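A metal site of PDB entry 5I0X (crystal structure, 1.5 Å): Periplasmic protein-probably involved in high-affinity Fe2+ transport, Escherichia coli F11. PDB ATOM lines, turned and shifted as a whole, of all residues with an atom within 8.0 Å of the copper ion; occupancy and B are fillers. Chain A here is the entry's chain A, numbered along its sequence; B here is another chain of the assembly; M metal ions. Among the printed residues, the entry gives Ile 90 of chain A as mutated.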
ATOM      1  N   VAL A  22      11.472 -21.212  -4.883  1.00  0.00           N
ATOM      2  CA  VAL A  22      10.722 -20.463  -3.877  1.00  0.00           C
ATOM      3  C   VAL A  22      11.466 -20.587  -2.574  1.00  0.00           C
ATOM      4  O   VAL A  22      12.235 -21.513  -2.363  1.00  0.00           O
ATOM      5  CB  VAL A  22       9.292 -21.012  -3.651  1.00  0.00           C
ATOM      6  CG1 VAL A  22       8.391 -20.761  -4.851  1.00  0.00           C
ATOM      7  CG2 VAL A  22       9.331 -22.485  -3.264  1.00  0.00           C
ATOM      8  N   LEU A  24      10.903 -19.893   1.908  1.00  0.00           N
ATOM      9  CA  LEU A  24       9.983 -19.647   3.017  1.00  0.00           C
ATOM     10  C   LEU A  24      10.807 -19.571   4.274  1.00  0.00           C
ATOM     11  O   LEU A  24      12.040 -19.571   4.214  1.00  0.00           O
ATOM     12  CB  LEU A  24       8.913 -20.726   3.083  1.00  0.00           C
ATOM     13  CG  LEU A  24       9.160 -22.202   2.858  1.00  0.00           C
ATOM     14  CD1 LEU A  24       7.986 -23.017   3.376  1.00  0.00           C
ATOM     15  CD2 LEU A  24       9.325 -22.484   1.369  1.00  0.00           C
ATOM     16  N   GLN A  25      10.120 -19.515   5.408  1.00  0.00           N
ATOM     17  CA  GLN A  25      10.727 -19.564   6.728  1.00  0.00           C
ATOM     18  C   GLN A  25      11.525 -20.868   6.916  1.00  0.00           C
ATOM     19  O   GLN A  25      11.154 -21.896   6.323  1.00  0.00           O
ATOM     20  CB  GLN A  25       9.613 -19.448   7.765  1.00  0.00           C
ATOM     21  CG  GLN A  25       8.362 -20.267   7.428  1.00  0.00           C
ATOM     22  CD  GLN A  25       7.566 -19.809   6.198  1.00  0.00           C
ATOM     23  OE1 GLN A  25       7.611 -18.641   5.786  1.00  0.00           O
ATOM     24  NE2 GLN A  25       6.804 -20.731   5.626  1.00  0.00           N
ATOM     25  N   ILE A  27      12.632 -24.434   8.069  1.00  0.00           N
ATOM     26  CA  ILE A  27      11.782 -25.552   8.461  1.00  0.00           C
ATOM     27  C   ILE A  27      12.634 -26.658   9.089  1.00  0.00           C
ATOM     28  O   ILE A  27      13.618 -27.079   8.518  1.00  0.00           O
ATOM     29  CB  ILE A  27      10.995 -26.069   7.229  1.00  0.00           C
ATOM     30  CG1 ILE A  27       9.975 -25.016   6.800  1.00  0.00           C
ATOM     31  CG2 ILE A  27      10.331 -27.416   7.526  1.00  0.00           C
ATOM     32  CD1 ILE A  27       9.077 -25.430   5.661  1.00  0.00           C
ATOM     33  N   MET A  29      13.620 -30.307   9.783  1.00  0.00           N
ATOM     34  CA  MET A  29      13.425 -31.510   8.993  1.00  0.00           C
ATOM     35  C   MET A  29      13.947 -32.730   9.719  1.00  0.00           C
ATOM     36  O   MET A  29      14.835 -32.612  10.577  1.00  0.00           O
ATOM     37  CB  MET A  29      14.095 -31.385   7.630  1.00  0.00           C
ATOM     38  CG  MET A  29      13.422 -30.364   6.716  1.00  0.00           C
ATOM     39  SD  MET A  29      14.196 -30.330   5.075  1.00  0.00           S
ATOM     40  CE  MET A  29      15.645 -29.371   5.537  1.00  0.00           C
ATOM     41  N   HIS A  44      14.215 -21.243   4.087  1.00  0.00           N
ATOM     42  CA  HIS A  44      14.221 -22.576   3.501  1.00  0.00           C
ATOM     43  C   HIS A  44      14.042 -22.388   2.025  1.00  0.00           C
ATOM     44  O   HIS A  44      13.050 -21.849   1.599  1.00  0.00           O
ATOM     45  CB  HIS A  44      13.087 -23.381   4.126  1.00  0.00           C
ATOM     46  CG  HIS A  44      13.001 -24.799   3.626  1.00  0.00           C
ATOM     47  ND1 HIS A  44      13.760 -25.807   4.117  1.00  0.00           N
ATOM     48  CD2 HIS A  44      12.153 -25.382   2.682  1.00  0.00           C
ATOM     49  CE1 HIS A  44      13.431 -26.958   3.491  1.00  0.00           C
ATOM     50  NE2 HIS A  44      12.456 -26.694   2.625  1.00  0.00           N
ATOM     51  N   LEU A  45      15.049 -22.780   1.226  1.00  0.00           N
ATOM     52  CA  LEU A  45      15.046 -22.592  -0.236  1.00  0.00           C
ATOM     53  C   LEU A  45      14.715 -23.911  -0.947  1.00  0.00           C
ATOM     54  O   LEU A  45      15.265 -24.965  -0.600  1.00  0.00           O
ATOM     55  CB  LEU A  45      16.405 -22.054  -0.690  1.00  0.00           C
ATOM     56  CG  LEU A  45      16.525 -21.696  -2.172  1.00  0.00           C
ATOM     57  CD1 LEU A  45      15.567 -20.586  -2.602  1.00  0.00           C
ATOM     58  CD2 LEU A  45      17.968 -21.329  -2.509  1.00  0.00           C
ATOM     59  N   GLU A  46      13.808 -23.818  -1.908  1.00  0.00           N
ATOM     60  CA  GLU A  46      13.249 -24.976  -2.637  1.00  0.00           C
ATOM     61  C   GLU A  46      13.536 -24.926  -4.136  1.00  0.00           C
ATOM     62  O   GLU A  46      13.635 -23.839  -4.737  1.00  0.00           O
ATOM     63  CB  GLU A  46      11.731 -25.022  -2.477  1.00  0.00           C
ATOM     64  CG  GLU A  46      11.204 -24.678  -1.102  1.00  0.00           C
ATOM     65  CD  GLU A  46      11.029 -25.894  -0.214  1.00  0.00           C
ATOM     66  OE1 GLU A  46      11.999 -26.675  -0.061  1.00  0.00           O
ATOM     67  OE2 GLU A  46       9.913 -26.067   0.347  1.00  0.00           O
ATOM     68  N   ALA A  47      13.639 -26.113  -4.729  1.00  0.00           N
ATOM     69  CA  ALA A  47      13.554 -26.272  -6.171  1.00  0.00           C
ATOM     70  C   ALA A  47      12.304 -27.099  -6.428  1.00  0.00           C
ATOM     71  O   ALA A  47      12.150 -28.192  -5.865  1.00  0.00           O
ATOM     72  CB  ALA A  47      14.783 -27.021  -6.708  1.00  0.00           C
ATOM     73  N   MET A  88      18.658 -31.335  -0.729  1.00  0.00           N
ATOM     74  CA  MET A  88      18.245 -32.687  -0.383  1.00  0.00           C
ATOM     75  C   MET A  88      16.871 -32.971  -0.986  1.00  0.00           C
ATOM     76  O   MET A  88      16.082 -32.034  -1.195  1.00  0.00           O
ATOM     77  CB  MET A  88      18.168 -32.818   1.134  1.00  0.00           C
ATOM     78  CG  MET A  88      19.517 -32.891   1.810  1.00  0.00           C
ATOM     79  SD  MET A  88      19.270 -32.635   3.569  1.00  0.00           S
ATOM     80  CE  MET A  88      18.457 -31.043   3.499  1.00  0.00           C
ATOM     81  N   PRO A  89      16.557 -34.246  -1.269  1.00  0.00           N
ATOM     82  CA  PRO A  89      15.166 -34.596  -1.594  1.00  0.00           C
ATOM     83  C   PRO A  89      14.367 -34.547  -0.301  1.00  0.00           C
ATOM     84  O   PRO A  89      14.854 -34.981   0.746  1.00  0.00           O
ATOM     85  CB  PRO A  89      15.250 -36.033  -2.135  1.00  0.00           C
ATOM     86  CG  PRO A  89      16.656 -36.479  -1.931  1.00  0.00           C
ATOM     87  CD  PRO A  89      17.454 -35.412  -1.265  1.00  0.00           C
ATOM     88  N   ILE A  90      13.165 -33.977  -0.379  1.00  0.00           N
ATOM     89  CA  ILE A  90      12.343 -33.680   0.820  1.00  0.00           C
ATOM     90  C   ILE A  90      10.887 -33.940   0.475  1.00  0.00           C
ATOM     91  O   ILE A  90      10.452 -33.643  -0.618  1.00  0.00           O
ATOM     92  CB  ILE A  90      12.474 -32.198   1.233  1.00  0.00           C
ATOM     93  CG1 ILE A  90      13.940 -31.804   1.435  1.00  0.00           C
ATOM     94  CG2 ILE A  90      11.677 -31.954   2.502  1.00  0.00           C
ATOM     95  CD1 ILE A  90      14.147 -30.304   1.481  1.00  0.00           C
ATOM     96  N   VAL A  91      10.128 -34.462   1.432  1.00  0.00           N
ATOM     97  CA  VAL A  91       8.685 -34.532   1.251  1.00  0.00           C
ATOM     98  C   VAL A  91       7.982 -33.631   2.250  1.00  0.00           C
ATOM     99  O   VAL A  91       8.364 -33.557   3.411  1.00  0.00           O
ATOM    100  CB  VAL A  91       8.144 -35.964   1.349  1.00  0.00           C
ATOM    101  CG1 VAL A  91       6.783 -36.051   0.682  1.00  0.00           C
ATOM    102  CG2 VAL A  91       9.127 -36.939   0.727  1.00  0.00           C
ATOM    103  N   ALA A  92       6.961 -32.952   1.752  1.00  0.00           N
ATOM    104  CA  ALA A  92       6.092 -32.112   2.568  1.00  0.00           C
ATOM    105  C   ALA A  92       4.667 -32.532   2.273  1.00  0.00           C
ATOM    106  O   ALA A  92       4.403 -33.415   1.447  1.00  0.00           O
ATOM    107  CB  ALA A  92       6.309 -30.662   2.193  1.00  0.00           C
ATOM    108  N   ASP A  94       2.374 -31.234   0.596  1.00  0.00           N
ATOM    109  CA  ASP A  94       1.942 -31.097  -0.786  1.00  0.00           C
ATOM    110  C   ASP A  94       2.909 -31.779  -1.763  1.00  0.00           C
ATOM    111  O   ASP A  94       2.858 -31.516  -2.969  1.00  0.00           O
ATOM    112  CB  ASP A  94       1.804 -29.632  -1.143  1.00  0.00           C
ATOM    113  CG  ASP A  94       3.140 -28.974  -1.293  1.00  0.00           C
ATOM    114  OD1 ASP A  94       4.048 -29.353  -0.528  1.00  0.00           O
ATOM    115  OD2 ASP A  94       3.300 -28.123  -2.202  1.00  0.00           O
ATOM    116  N   GLY A  95       3.788 -32.649  -1.258  1.00  0.00           N
ATOM    117  CA  GLY A  95       4.535 -33.507  -2.147  1.00  0.00           C
ATOM    118  C   GLY A  95       6.046 -33.388  -2.046  1.00  0.00           C
ATOM    119  O   GLY A  95       6.589 -32.567  -1.299  1.00  0.00           O
ATOM    120  N   PRO A  96       6.729 -34.205  -2.847  1.00  0.00           N
ATOM    121  CA  PRO A  96       8.188 -34.210  -2.894  1.00  0.00           C
ATOM    122  C   PRO A  96       8.755 -32.970  -3.602  1.00  0.00           C
ATOM    123  O   PRO A  96       8.151 -32.423  -4.535  1.00  0.00           O
ATOM    124  CB  PRO A  96       8.492 -35.473  -3.670  1.00  0.00           C
ATOM    125  CG  PRO A  96       7.320 -35.633  -4.598  1.00  0.00           C
ATOM    126  CD  PRO A  96       6.155 -35.239  -3.712  1.00  0.00           C
ATOM    127  N   HIS A  97       9.910 -32.541  -3.126  1.00  0.00           N
ATOM    128  CA  HIS A  97      10.651 -31.437  -3.741  1.00  0.00           C
ATOM    129  C   HIS A  97      12.095 -31.569  -3.359  1.00  0.00           C
ATOM    130  O   HIS A  97      12.507 -32.613  -2.807  1.00  0.00           O
ATOM    131  CB  HIS A  97      10.090 -30.074  -3.304  1.00  0.00           C
ATOM    132  CG  HIS A  97      10.153 -29.809  -1.810  1.00  0.00           C
ATOM    133  ND1 HIS A  97       9.240 -30.289  -0.953  1.00  0.00           N
ATOM    134  CD2 HIS A  97      11.054 -29.070  -1.055  1.00  0.00           C
ATOM    135  CE1 HIS A  97       9.557 -29.893   0.306  1.00  0.00           C
ATOM    136  NE2 HIS A  97      10.659 -29.127   0.236  1.00  0.00           N
ATOM    137  N   TYR A  98      12.906 -30.558  -3.702  1.00  0.00           N
ATOM    138  CA  TYR A  98      14.301 -30.531  -3.264  1.00  0.00           C
ATOM    139  C   TYR A  98      14.506 -29.214  -2.531  1.00  0.00           C
ATOM    140  O   TYR A  98      13.877 -28.206  -2.888  1.00  0.00           O
ATOM    141  CB  TYR A  98      15.248 -30.558  -4.469  1.00  0.00           C
ATOM    142  CG  TYR A  98      15.128 -31.783  -5.305  1.00  0.00           C
ATOM    143  CD1 TYR A  98      15.845 -32.930  -4.976  1.00  0.00           C
ATOM    144  CD2 TYR A  98      14.258 -31.819  -6.411  1.00  0.00           C
ATOM    145  CE1 TYR A  98      15.729 -34.088  -5.755  1.00  0.00           C
ATOM    146  CE2 TYR A  98      14.135 -32.961  -7.191  1.00  0.00           C
ATOM    147  CZ  TYR A  98      14.870 -34.095  -6.863  1.00  0.00           C
ATOM    148  OH  TYR A  98      14.737 -35.216  -7.652  1.00  0.00           O
ATOM    149  N   GLY A  99      15.400 -29.186  -1.551  1.00  0.00           N
ATOM    150  CA  GLY A  99      15.638 -27.939  -0.856  1.00  0.00           C
ATOM    151  C   GLY A  99      16.655 -28.035   0.246  1.00  0.00           C
ATOM    152  O   GLY A  99      17.294 -29.067   0.428  1.00  0.00           O
ATOM    153  N   ALA A 100      16.798 -26.926   0.963  1.00  0.00           N
ATOM    154  CA  ALA A 100      17.718 -26.846   2.116  1.00  0.00           C
ATOM    155  C   ALA A 100      17.363 -25.609   2.927  1.00  0.00           C
ATOM    156  O   ALA A 100      16.928 -24.587   2.376  1.00  0.00           O
ATOM    157  CB  ALA A 100      19.159 -26.719   1.645  1.00  0.00           C
ATOM    158  N   ASN A 101      17.628 -25.677   4.229  1.00  0.00           N
ATOM    159  CA  ASN A 101      17.697 -24.463   5.035  1.00  0.00           C
ATOM    160  C   ASN A 101      19.007 -23.730   4.728  1.00  0.00           C
ATOM    161  O   ASN A 101      20.081 -24.357   4.619  1.00  0.00           O
ATOM    162  CB  ASN A 101      17.629 -24.797   6.542  1.00  0.00           C
ATOM    163  CG  ASN A 101      16.292 -25.366   6.970  1.00  0.00           C
ATOM    164  OD1 ASN A 101      16.240 -26.268   7.825  1.00  0.00           O
ATOM    165  ND2 ASN A 101      15.213 -24.852   6.414  1.00  0.00           N
ATOM    166  N   HIS B 125      14.348 -36.487   3.105  1.00  0.00           N
ATOM    167  CA  HIS B 125      13.994 -35.814   4.359  1.00  0.00           C
ATOM    168  C   HIS B 125      12.555 -35.416   4.341  1.00  0.00           C
ATOM    169  O   HIS B 125      11.860 -35.580   3.343  1.00  0.00           O
ATOM    170  CB  HIS B 125      14.886 -34.596   4.546  1.00  0.00           C
ATOM    171  CG  HIS B 125      16.297 -34.937   4.898  1.00  0.00           C
ATOM    172  ND1 HIS B 125      17.126 -35.595   4.060  1.00  0.00           N
ATOM    173  CD2 HIS B 125      17.043 -34.662   6.050  1.00  0.00           C
ATOM    174  CE1 HIS B 125      18.330 -35.753   4.652  1.00  0.00           C
ATOM    175  NE2 HIS B 125      18.276 -35.189   5.867  1.00  0.00           N
ATOM    176  N   ARG B 126      12.059 -34.903   5.471  1.00  0.00           N
ATOM    177  CA  ARG B 126      10.663 -34.469   5.549  1.00  0.00           C
ATOM    178  C   ARG B 126      10.518 -33.176   6.351  1.00  0.00           C
ATOM    179  O   ARG B 126      11.172 -33.020   7.388  1.00  0.00           O
ATOM    180  CB  ARG B 126       9.749 -35.572   6.137  1.00  0.00           C
ATOM    181  CG  ARG B 126      10.105 -36.080   7.525  1.00  0.00           C
ATOM    182  CD  ARG B 126       9.207 -37.243   7.929  1.00  0.00           C
ATOM    183  NE  ARG B 126       9.754 -37.812   9.147  1.00  0.00           N
ATOM    184  CZ  ARG B 126       9.379 -37.426  10.362  1.00  0.00           C
ATOM    185  NH1 ARG B 126       9.935 -37.955  11.437  1.00  0.00           N
ATOM    186  NH2 ARG B 126       8.415 -36.525  10.498  1.00  0.00           N
ATOM    187  N   HIS B 127       9.637 -32.292   5.891  1.00  0.00           N
ATOM    188  CA  HIS B 127       9.217 -31.137   6.715  1.00  0.00           C
ATOM    189  C   HIS B 127       8.546 -31.658   7.949  1.00  0.00           C
ATOM    190  O   HIS B 127       7.809 -32.654   7.887  1.00  0.00           O
ATOM    191  CB  HIS B 127       8.214 -30.258   5.970  1.00  0.00           C
ATOM    192  CG  HIS B 127       8.816 -29.447   4.831  1.00  0.00           C
ATOM    193  ND1 HIS B 127       8.126 -28.453   4.227  1.00  0.00           N
ATOM    194  CD2 HIS B 127      10.054 -29.520   4.208  1.00  0.00           C
ATOM    195  CE1 HIS B 127       8.898 -27.920   3.245  1.00  0.00           C
ATOM    196  NE2 HIS B 127      10.082 -28.577   3.238  1.00  0.00           N
ATOM    197  N   ASP B 129       7.228 -29.007  10.242  1.00  0.00           N
ATOM    198  CA  ASP B 129       6.408 -27.877  10.707  1.00  0.00           C
ATOM    199  C   ASP B 129       4.910 -28.217  10.706  1.00  0.00           C
ATOM    200  O   ASP B 129       4.487 -29.134  10.025  1.00  0.00           O
ATOM    201  CB  ASP B 129       6.664 -26.632   9.844  1.00  0.00           C
ATOM    202  CG  ASP B 129       6.167 -26.813   8.416  1.00  0.00           C
ATOM    203  OD1 ASP B 129       6.770 -27.622   7.681  1.00  0.00           O
ATOM    204  OD2 ASP B 129       5.178 -26.133   8.037  1.00  0.00           O
ATOM    205  N   THR B 132       3.194 -27.502   6.828  1.00  0.00           N
ATOM    206  CA  THR B 132       3.557 -28.359   5.682  1.00  0.00           C
ATOM    207  C   THR B 132       4.187 -29.698   6.041  1.00  0.00           C
ATOM    208  O   THR B 132       4.608 -30.448   5.154  1.00  0.00           O
ATOM    209  CB  THR B 132       4.491 -27.633   4.685  1.00  0.00           C
ATOM    210  OG1 THR B 132       5.774 -27.438   5.286  1.00  0.00           O
ATOM    211  CG2 THR B 132       3.906 -26.271   4.267  1.00  0.00           C
HETATM  212 CU    CU M   1      11.344 -27.971   1.671  1.00  0.00          CU
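NE2 of His 44 is bound to the copper ion, at 1.9 Å.
NE2 of His 97 binds the copper ion, 2.0 Å away.
NE2 of His 127 of chain B binds the copper ion (2.1 Å).
The copper ion is bound by OE1 of Glu 46.
Slightly farther from the copper ion lies OE2 of Glu 46 (2.7 Å).
O of Val 22 sits at hydrogen-bond distance from N of Glu 46, 2.8 Å away.
N of His 127 of chain B is in hydrogen-bond range of O of Val 91 (3.1 Å).
OG1 of Thr 132 of chain B is in hydrogen-bond range of ND1 of His 127 of chain B (2.8 Å).
The backbone NH of His 97 lies within hydrogen-bond range of the backbone carbonyl oxygen of Ile 90.
N of His 44 lies within hydrogen-bond range of O of Leu 24.
ND2 of Asn 101 sits at hydrogen-bond distance from ND1 of His 44 (2.9 Å).
Merely in contact with the copper ion: Ile 90.
Of the 27 residues printed, 5 come within 4 Å of the copper ion.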
